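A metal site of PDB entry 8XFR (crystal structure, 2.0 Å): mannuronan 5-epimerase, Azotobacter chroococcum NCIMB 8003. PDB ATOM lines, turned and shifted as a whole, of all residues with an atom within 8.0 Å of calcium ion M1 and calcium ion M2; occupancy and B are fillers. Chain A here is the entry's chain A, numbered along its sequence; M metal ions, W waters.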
ATOM      1  N   VAL A 330      -5.712  23.273 -34.243  1.00  0.00           N
ATOM      2  CA  VAL A 330      -7.083  23.271 -33.726  1.00  0.00           C
ATOM      3  C   VAL A 330      -7.036  23.931 -32.366  1.00  0.00           C
ATOM      4  O   VAL A 330      -6.509  23.351 -31.406  1.00  0.00           O
ATOM      5  CB  VAL A 330      -7.702  21.870 -33.619  1.00  0.00           C
ATOM      6  CG1 VAL A 330      -9.214  21.966 -33.347  1.00  0.00           C
ATOM      7  CG2 VAL A 330      -7.469  21.076 -34.897  1.00  0.00           C
ATOM      8  N   GLY A 332      -8.925  24.347 -29.761  1.00  0.00           N
ATOM      9  CA  GLY A 332     -10.106  23.871 -29.069  1.00  0.00           C
ATOM     10  C   GLY A 332     -10.178  22.366 -29.211  1.00  0.00           C
ATOM     11  O   GLY A 332      -9.301  21.730 -29.795  1.00  0.00           O
ATOM     12  N   ALA A 333     -11.250  21.802 -28.664  1.00  0.00           N
ATOM     13  CA  ALA A 333     -11.297  20.358 -28.476  1.00  0.00           C
ATOM     14  C   ALA A 333     -11.718  19.624 -29.738  1.00  0.00           C
ATOM     15  O   ALA A 333     -12.666  20.017 -30.439  1.00  0.00           O
ATOM     16  CB  ALA A 333     -12.252  20.011 -27.336  1.00  0.00           C
ATOM     17  N   ALA A 334     -11.044  18.510 -30.014  1.00  0.00           N
ATOM     18  CA  ALA A 334     -11.387  17.638 -31.142  1.00  0.00           C
ATOM     19  C   ALA A 334     -11.944  16.331 -30.603  1.00  0.00           C
ATOM     20  O   ALA A 334     -11.300  15.678 -29.771  1.00  0.00           O
ATOM     21  CB  ALA A 334     -10.164  17.374 -32.027  1.00  0.00           C
ATOM     22  N   ASP A 346      -4.894  12.264 -34.766  1.00  0.00           N
ATOM     23  CA  ASP A 346      -3.994  13.171 -34.070  1.00  0.00           C
ATOM     24  C   ASP A 346      -4.842  14.330 -33.573  1.00  0.00           C
ATOM     25  O   ASP A 346      -5.473  15.013 -34.381  1.00  0.00           O
ATOM     26  CB  ASP A 346      -2.891  13.707 -35.008  1.00  0.00           C
ATOM     27  CG  ASP A 346      -1.908  12.632 -35.460  1.00  0.00           C
ATOM     28  OD1 ASP A 346      -1.138  12.928 -36.398  1.00  0.00           O
ATOM     29  OD2 ASP A 346      -1.877  11.497 -34.878  1.00  0.00           O
ATOM     30  N   GLY A 347      -4.838  14.551 -32.259  1.00  0.00           N
ATOM     31  CA  GLY A 347      -5.404  15.770 -31.724  1.00  0.00           C
ATOM     32  C   GLY A 347      -4.431  16.936 -31.900  1.00  0.00           C
ATOM     33  O   GLY A 347      -3.360  16.809 -32.496  1.00  0.00           O
ATOM     34  N   ALA A 348      -4.790  18.081 -31.345  1.00  0.00           N
ATOM     35  CA  ALA A 348      -4.000  19.322 -31.463  1.00  0.00           C
ATOM     36  C   ALA A 348      -4.010  19.986 -30.090  1.00  0.00           C
ATOM     37  O   ALA A 348      -3.983  19.315 -29.054  1.00  0.00           O
ATOM     38  CB  ALA A 348      -4.487  20.211 -32.613  1.00  0.00           C
ATOM     39  N   ALA A 349      -3.886  21.325 -30.061  1.00  0.00           N
ATOM     40  CA  ALA A 349      -3.669  22.054 -28.811  1.00  0.00           C
ATOM     41  C   ALA A 349      -4.783  21.866 -27.784  1.00  0.00           C
ATOM     42  O   ALA A 349      -4.556  22.111 -26.587  1.00  0.00           O
ATOM     43  CB  ALA A 349      -3.484  23.556 -29.106  1.00  0.00           C
ATOM     44  N   GLY A 350      -5.981  21.447 -28.189  1.00  0.00           N
ATOM     45  CA  GLY A 350      -7.098  21.346 -27.267  1.00  0.00           C
ATOM     46  C   GLY A 350      -7.056  20.080 -26.416  1.00  0.00           C
ATOM     47  O   GLY A 350      -6.181  19.232 -26.531  1.00  0.00           O
ATOM     48  N   ASN A 351      -8.048  19.968 -25.524  1.00  0.00           N
ATOM     49  CA  ASN A 351      -8.224  18.800 -24.668  1.00  0.00           C
ATOM     50  C   ASN A 351      -9.130  17.836 -25.421  1.00  0.00           C
ATOM     51  O   ASN A 351     -10.344  17.965 -25.386  1.00  0.00           O
ATOM     52  CB  ASN A 351      -8.850  19.175 -23.324  1.00  0.00           C
ATOM     53  CG  ASN A 351      -7.885  19.872 -22.394  1.00  0.00           C
ATOM     54  OD1 ASN A 351      -6.724  20.131 -22.719  1.00  0.00           O
ATOM     55  ND2 ASN A 351      -8.361  20.155 -21.202  1.00  0.00           N
ATOM     56  N   ASP A 352      -8.526  16.880 -26.120  1.00  0.00           N
ATOM     57  CA  ASP A 352      -9.220  16.074 -27.109  1.00  0.00           C
ATOM     58  C   ASP A 352      -9.642  14.716 -26.566  1.00  0.00           C
ATOM     59  O   ASP A 352      -9.059  14.182 -25.612  1.00  0.00           O
ATOM     60  CB  ASP A 352      -8.339  15.891 -28.349  1.00  0.00           C
ATOM     61  CG  ASP A 352      -7.725  17.204 -28.825  1.00  0.00           C
ATOM     62  OD1 ASP A 352      -8.471  18.190 -28.974  1.00  0.00           O
ATOM     63  OD2 ASP A 352      -6.507  17.242 -29.064  1.00  0.00           O
ATOM     64  N   LEU A 353     -10.660  14.144 -27.204  1.00  0.00           N
ATOM     65  CA  LEU A 353     -11.113  12.774 -26.941  1.00  0.00           C
ATOM     66  C   LEU A 353     -10.810  11.933 -28.168  1.00  0.00           C
ATOM     67  O   LEU A 353     -11.296  12.252 -29.260  1.00  0.00           O
ATOM     68  CB  LEU A 353     -12.618  12.739 -26.637  1.00  0.00           C
ATOM     69  CG  LEU A 353     -13.268  11.358 -26.553  1.00  0.00           C
ATOM     70  CD1 LEU A 353     -12.712  10.582 -25.377  1.00  0.00           C
ATOM     71  CD2 LEU A 353     -14.797  11.414 -26.444  1.00  0.00           C
ATOM     72  N   LEU A 354     -10.049  10.849 -27.993  1.00  0.00           N
ATOM     73  CA  LEU A 354      -9.638  10.003 -29.101  1.00  0.00           C
ATOM     74  C   LEU A 354     -10.083   8.571 -28.878  1.00  0.00           C
ATOM     75  O   LEU A 354      -9.841   7.999 -27.811  1.00  0.00           O
ATOM     76  CB  LEU A 354      -8.111  10.029 -29.293  1.00  0.00           C
ATOM     77  CG  LEU A 354      -7.673  11.437 -29.717  1.00  0.00           C
ATOM     78  CD1 LEU A 354      -7.108  12.155 -28.513  1.00  0.00           C
ATOM     79  CD2 LEU A 354      -6.644  11.327 -30.820  1.00  0.00           C
ATOM     80  N   SER A 364      -2.598  10.142 -31.252  1.00  0.00           N
ATOM     81  CA  SER A 364      -1.746  11.075 -30.549  1.00  0.00           C
ATOM     82  C   SER A 364      -2.595  12.233 -30.052  1.00  0.00           C
ATOM     83  O   SER A 364      -3.580  12.622 -30.693  1.00  0.00           O
ATOM     84  CB  SER A 364      -0.613  11.571 -31.441  1.00  0.00           C
ATOM     85  OG  SER A 364      -1.099  12.557 -32.329  1.00  0.00           O
ATOM     86  N   GLY A 365      -2.234  12.759 -28.885  1.00  0.00           N
ATOM     87  CA  GLY A 365      -3.011  13.829 -28.322  1.00  0.00           C
ATOM     88  C   GLY A 365      -2.537  15.222 -28.727  1.00  0.00           C
ATOM     89  O   GLY A 365      -3.343  16.156 -28.748  1.00  0.00           O
ATOM     90  N   GLY A 366      -1.233  15.378 -29.014  1.00  0.00           N
ATOM     91  CA  GLY A 366      -0.771  16.749 -29.140  1.00  0.00           C
ATOM     92  C   GLY A 366      -0.794  17.475 -27.800  1.00  0.00           C
ATOM     93  O   GLY A 366      -0.829  16.862 -26.723  1.00  0.00           O
ATOM     94  N   GLY A 367      -0.806  18.808 -27.877  1.00  0.00           N
ATOM     95  CA  GLY A 367      -0.801  19.628 -26.679  1.00  0.00           C
ATOM     96  C   GLY A 367      -2.063  19.408 -25.859  1.00  0.00           C
ATOM     97  O   GLY A 367      -2.994  18.723 -26.272  1.00  0.00           O
ATOM     98  N   GLY A 368      -2.074  19.953 -24.648  1.00  0.00           N
ATOM     99  CA  GLY A 368      -3.245  19.838 -23.800  1.00  0.00           C
ATOM    100  C   GLY A 368      -3.424  18.458 -23.161  1.00  0.00           C
ATOM    101  O   GLY A 368      -2.597  17.552 -23.304  1.00  0.00           O
ATOM    102  N   ALA A 369      -4.534  18.308 -22.455  1.00  0.00           N
ATOM    103  CA  ALA A 369      -4.815  17.115 -21.683  1.00  0.00           C
ATOM    104  C   ALA A 369      -5.841  16.277 -22.443  1.00  0.00           C
ATOM    105  O   ALA A 369      -7.007  16.644 -22.539  1.00  0.00           O
ATOM    106  CB  ALA A 369      -5.333  17.488 -20.297  1.00  0.00           C
ATOM    107  N   ASP A 370      -5.411  15.126 -22.951  1.00  0.00           N
ATOM    108  CA  ASP A 370      -6.224  14.323 -23.858  1.00  0.00           C
ATOM    109  C   ASP A 370      -6.607  13.003 -23.227  1.00  0.00           C
ATOM    110  O   ASP A 370      -5.817  12.395 -22.482  1.00  0.00           O
ATOM    111  CB  ASP A 370      -5.490  14.090 -25.163  1.00  0.00           C
ATOM    112  CG  ASP A 370      -5.031  15.392 -25.791  1.00  0.00           C
ATOM    113  OD1 ASP A 370      -5.876  16.230 -26.145  1.00  0.00           O
ATOM    114  OD2 ASP A 370      -3.824  15.584 -25.889  1.00  0.00           O
ATOM    115  N   THR A 371      -7.835  12.562 -23.530  1.00  0.00           N
ATOM    116  CA  THR A 371      -8.370  11.292 -23.080  1.00  0.00           C
ATOM    117  C   THR A 371      -8.357  10.329 -24.271  1.00  0.00           C
ATOM    118  O   THR A 371      -8.950  10.616 -25.315  1.00  0.00           O
ATOM    119  CB  THR A 371      -9.792  11.466 -22.549  1.00  0.00           C
ATOM    120  OG1 THR A 371      -9.758  12.257 -21.349  1.00  0.00           O
ATOM    121  CG2 THR A 371     -10.405  10.126 -22.233  1.00  0.00           C
ATOM    122  N   PHE A 372      -7.643   9.211 -24.106  1.00  0.00           N
ATOM    123  CA  PHE A 372      -7.665   8.100 -25.061  1.00  0.00           C
ATOM    124  C   PHE A 372      -8.617   7.050 -24.525  1.00  0.00           C
ATOM    125  O   PHE A 372      -8.335   6.405 -23.510  1.00  0.00           O
ATOM    126  CB  PHE A 372      -6.254   7.541 -25.254  1.00  0.00           C
ATOM    127  CG  PHE A 372      -5.254   8.594 -25.636  1.00  0.00           C
ATOM    128  CD1 PHE A 372      -4.566   9.306 -24.657  1.00  0.00           C
ATOM    129  CD2 PHE A 372      -5.033   8.907 -26.968  1.00  0.00           C
ATOM    130  CE1 PHE A 372      -3.663  10.303 -25.015  1.00  0.00           C
ATOM    131  CE2 PHE A 372      -4.123   9.897 -27.328  1.00  0.00           C
ATOM    132  CZ  PHE A 372      -3.442  10.603 -26.345  1.00  0.00           C
ATOM    133  N   ASP A 396       2.108   9.757 -27.961  1.00  0.00           N
ATOM    134  CA  ASP A 396       2.683  10.833 -27.146  1.00  0.00           C
ATOM    135  C   ASP A 396       2.013  10.920 -25.777  1.00  0.00           C
ATOM    136  O   ASP A 396       1.715  12.012 -25.285  1.00  0.00           O
ATOM    137  CB  ASP A 396       2.576  12.184 -27.859  1.00  0.00           C
ATOM    138  CG  ASP A 396       1.117  12.562 -28.171  1.00  0.00           C
ATOM    139  OD1 ASP A 396       0.231  11.680 -28.083  1.00  0.00           O
ATOM    140  OD2 ASP A 396       0.858  13.737 -28.532  1.00  0.00           O
ATOM    141  N   PHE A 397       1.766   9.786 -25.145  1.00  0.00           N
ATOM    142  CA  PHE A 397       1.059   9.841 -23.877  1.00  0.00           C
ATOM    143  C   PHE A 397       1.879  10.609 -22.850  1.00  0.00           C
ATOM    144  O   PHE A 397       3.069  10.359 -22.667  1.00  0.00           O
ATOM    145  CB  PHE A 397       0.751   8.442 -23.323  1.00  0.00           C
ATOM    146  CG  PHE A 397      -0.189   8.481 -22.174  1.00  0.00           C
ATOM    147  CD1 PHE A 397      -1.540   8.586 -22.395  1.00  0.00           C
ATOM    148  CD2 PHE A 397       0.276   8.489 -20.878  1.00  0.00           C
ATOM    149  CE1 PHE A 397      -2.433   8.660 -21.345  1.00  0.00           C
ATOM    150  CE2 PHE A 397      -0.596   8.564 -19.815  1.00  0.00           C
ATOM    151  CZ  PHE A 397      -1.952   8.653 -20.043  1.00  0.00           C
ATOM    152  N   THR A 398       1.223  11.538 -22.160  1.00  0.00           N
ATOM    153  CA  THR A 398       1.912  12.417 -21.220  1.00  0.00           C
ATOM    154  C   THR A 398       1.429  12.135 -19.804  1.00  0.00           C
ATOM    155  O   THR A 398       0.327  12.586 -19.424  1.00  0.00           O
ATOM    156  CB  THR A 398       1.673  13.869 -21.584  1.00  0.00           C
ATOM    157  OG1 THR A 398       1.978  14.055 -22.981  1.00  0.00           O
ATOM    158  CG2 THR A 398       2.550  14.761 -20.734  1.00  0.00           C
ATOM    159  N   ALA A 401      -0.767  14.457 -17.451  1.00  0.00           N
ATOM    160  CA  ALA A 401      -1.589  15.324 -18.307  1.00  0.00           C
ATOM    161  C   ALA A 401      -2.686  14.547 -19.011  1.00  0.00           C
ATOM    162  O   ALA A 401      -3.875  14.875 -18.854  1.00  0.00           O
ATOM    163  CB  ALA A 401      -0.708  16.030 -19.344  1.00  0.00           C
ATOM    164  N   ASP A 402      -2.339  13.514 -19.757  1.00  0.00           N
ATOM    165  CA  ASP A 402      -3.314  12.758 -20.526  1.00  0.00           C
ATOM    166  C   ASP A 402      -3.980  11.700 -19.640  1.00  0.00           C
ATOM    167  O   ASP A 402      -3.574  11.449 -18.499  1.00  0.00           O
ATOM    168  CB  ASP A 402      -2.648  12.099 -21.736  1.00  0.00           C
ATOM    169  CG  ASP A 402      -2.046  13.114 -22.711  1.00  0.00           C
ATOM    170  OD1 ASP A 402      -2.578  14.240 -22.843  1.00  0.00           O
ATOM    171  OD2 ASP A 402      -1.043  12.754 -23.375  1.00  0.00           O
ATOM    172  N   LEU A 403      -5.007  11.060 -20.191  1.00  0.00           N
ATOM    173  CA  LEU A 403      -5.748  10.011 -19.493  1.00  0.00           C
ATOM    174  C   LEU A 403      -6.122   8.878 -20.440  1.00  0.00           C
ATOM    175  O   LEU A 403      -6.603   9.129 -21.560  1.00  0.00           O
ATOM    176  CB  LEU A 403      -7.021  10.576 -18.847  1.00  0.00           C
ATOM    177  CG  LEU A 403      -7.907   9.556 -18.156  1.00  0.00           C
ATOM    178  CD1 LEU A 403      -7.248   9.118 -16.852  1.00  0.00           C
ATOM    179  CD2 LEU A 403      -9.312  10.139 -17.935  1.00  0.00           C
ATOM    180  N   THR A 476     -10.407  14.448 -18.778  1.00  0.00           N
ATOM    181  CA  THR A 476      -9.746  15.666 -19.188  1.00  0.00           C
ATOM    182  C   THR A 476     -10.602  16.520 -20.105  1.00  0.00           C
ATOM    183  O   THR A 476     -10.250  17.666 -20.368  1.00  0.00           O
ATOM    184  CB  THR A 476      -8.430  15.319 -19.897  1.00  0.00           C
ATOM    185  OG1 THR A 476      -8.714  14.854 -21.232  1.00  0.00           O
ATOM    186  CG2 THR A 476      -7.646  14.254 -19.103  1.00  0.00           C
HETATM  187 CA    CA M   1      -1.691  15.796 -24.732  1.00  0.00          CA
HETATM  188 CA    CA M   2      -4.701  17.686 -27.620  1.00  0.00          CA
HETATM  189  O   HOH W   1       0.639  16.038 -23.757  1.00  0.00           O
HETATM  190  O   HOH W   2      -0.874  13.469 -25.738  1.00  0.00           O
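The backbone carbonyl oxygen (O) of Gly 366 is bound to calcium ion M1, 2.4 Å away. OD2 of Asp 370 is bound to calcium ion M1. Calcium ion M1 is bound by the backbone carbonyl oxygen (O) of Gly 368 (2.4 Å). Water W1 binds calcium ion M1, 2.5 Å away. The side-chain carboxylate (OD1) of Asp 402 is bound to calcium ion M1, at 2.6 Å. Water W2 binds calcium ion M1 (2.7 Å).
Calcium ion M2 is bound by O of Ala 348 (2.3 Å), O of Gly 365 (2.3 Å), OD2 of Asp 352 (2.4 Å), OD1 of Asp 370 (2.4 Å), O of Gly 350 (2.4 Å), O of Gly 367 (2.4 Å) and OD2 of Asp 370 (2.9 Å). Calcium ion M2 has seven donor atoms within binding distance.
Of the 29 residues printed, 5 come within 4 Å of calcium ion M1. The nearest printed residue that does not touch calcium ion M1 is Gly 365 (4.1 Å).
Water W2 lies within hydrogen-bond range of OD2 of Asp 402 (2.5 Å) and O of Asp 396 (3.0 Å).
The backbone NH (N) of Gly 365 is in hydrogen-bond range of the side-chain carboxylate (OD1) of Asp 396. N of Ala 334 sits at hydrogen-bond distance from OD1 of Asp 352 (2.8 Å). The backbone NH (N) of Thr 371 sits at hydrogen-bond distance from the backbone carbonyl oxygen (O) of Asp 352, 2.9 Å away. N of Leu 403 lies within hydrogen-bond range of O of Asp 370 (2.8 Å). The backbone NH (N) of Gly 366 is in hydrogen-bond range of the side-chain carboxylate (OD2) of Asp 396 (2.7 Å). The side-chain carboxylate of Asp 402 is in hydrogen-bond range of the backbone NH of Thr 398 (2.8 Å).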
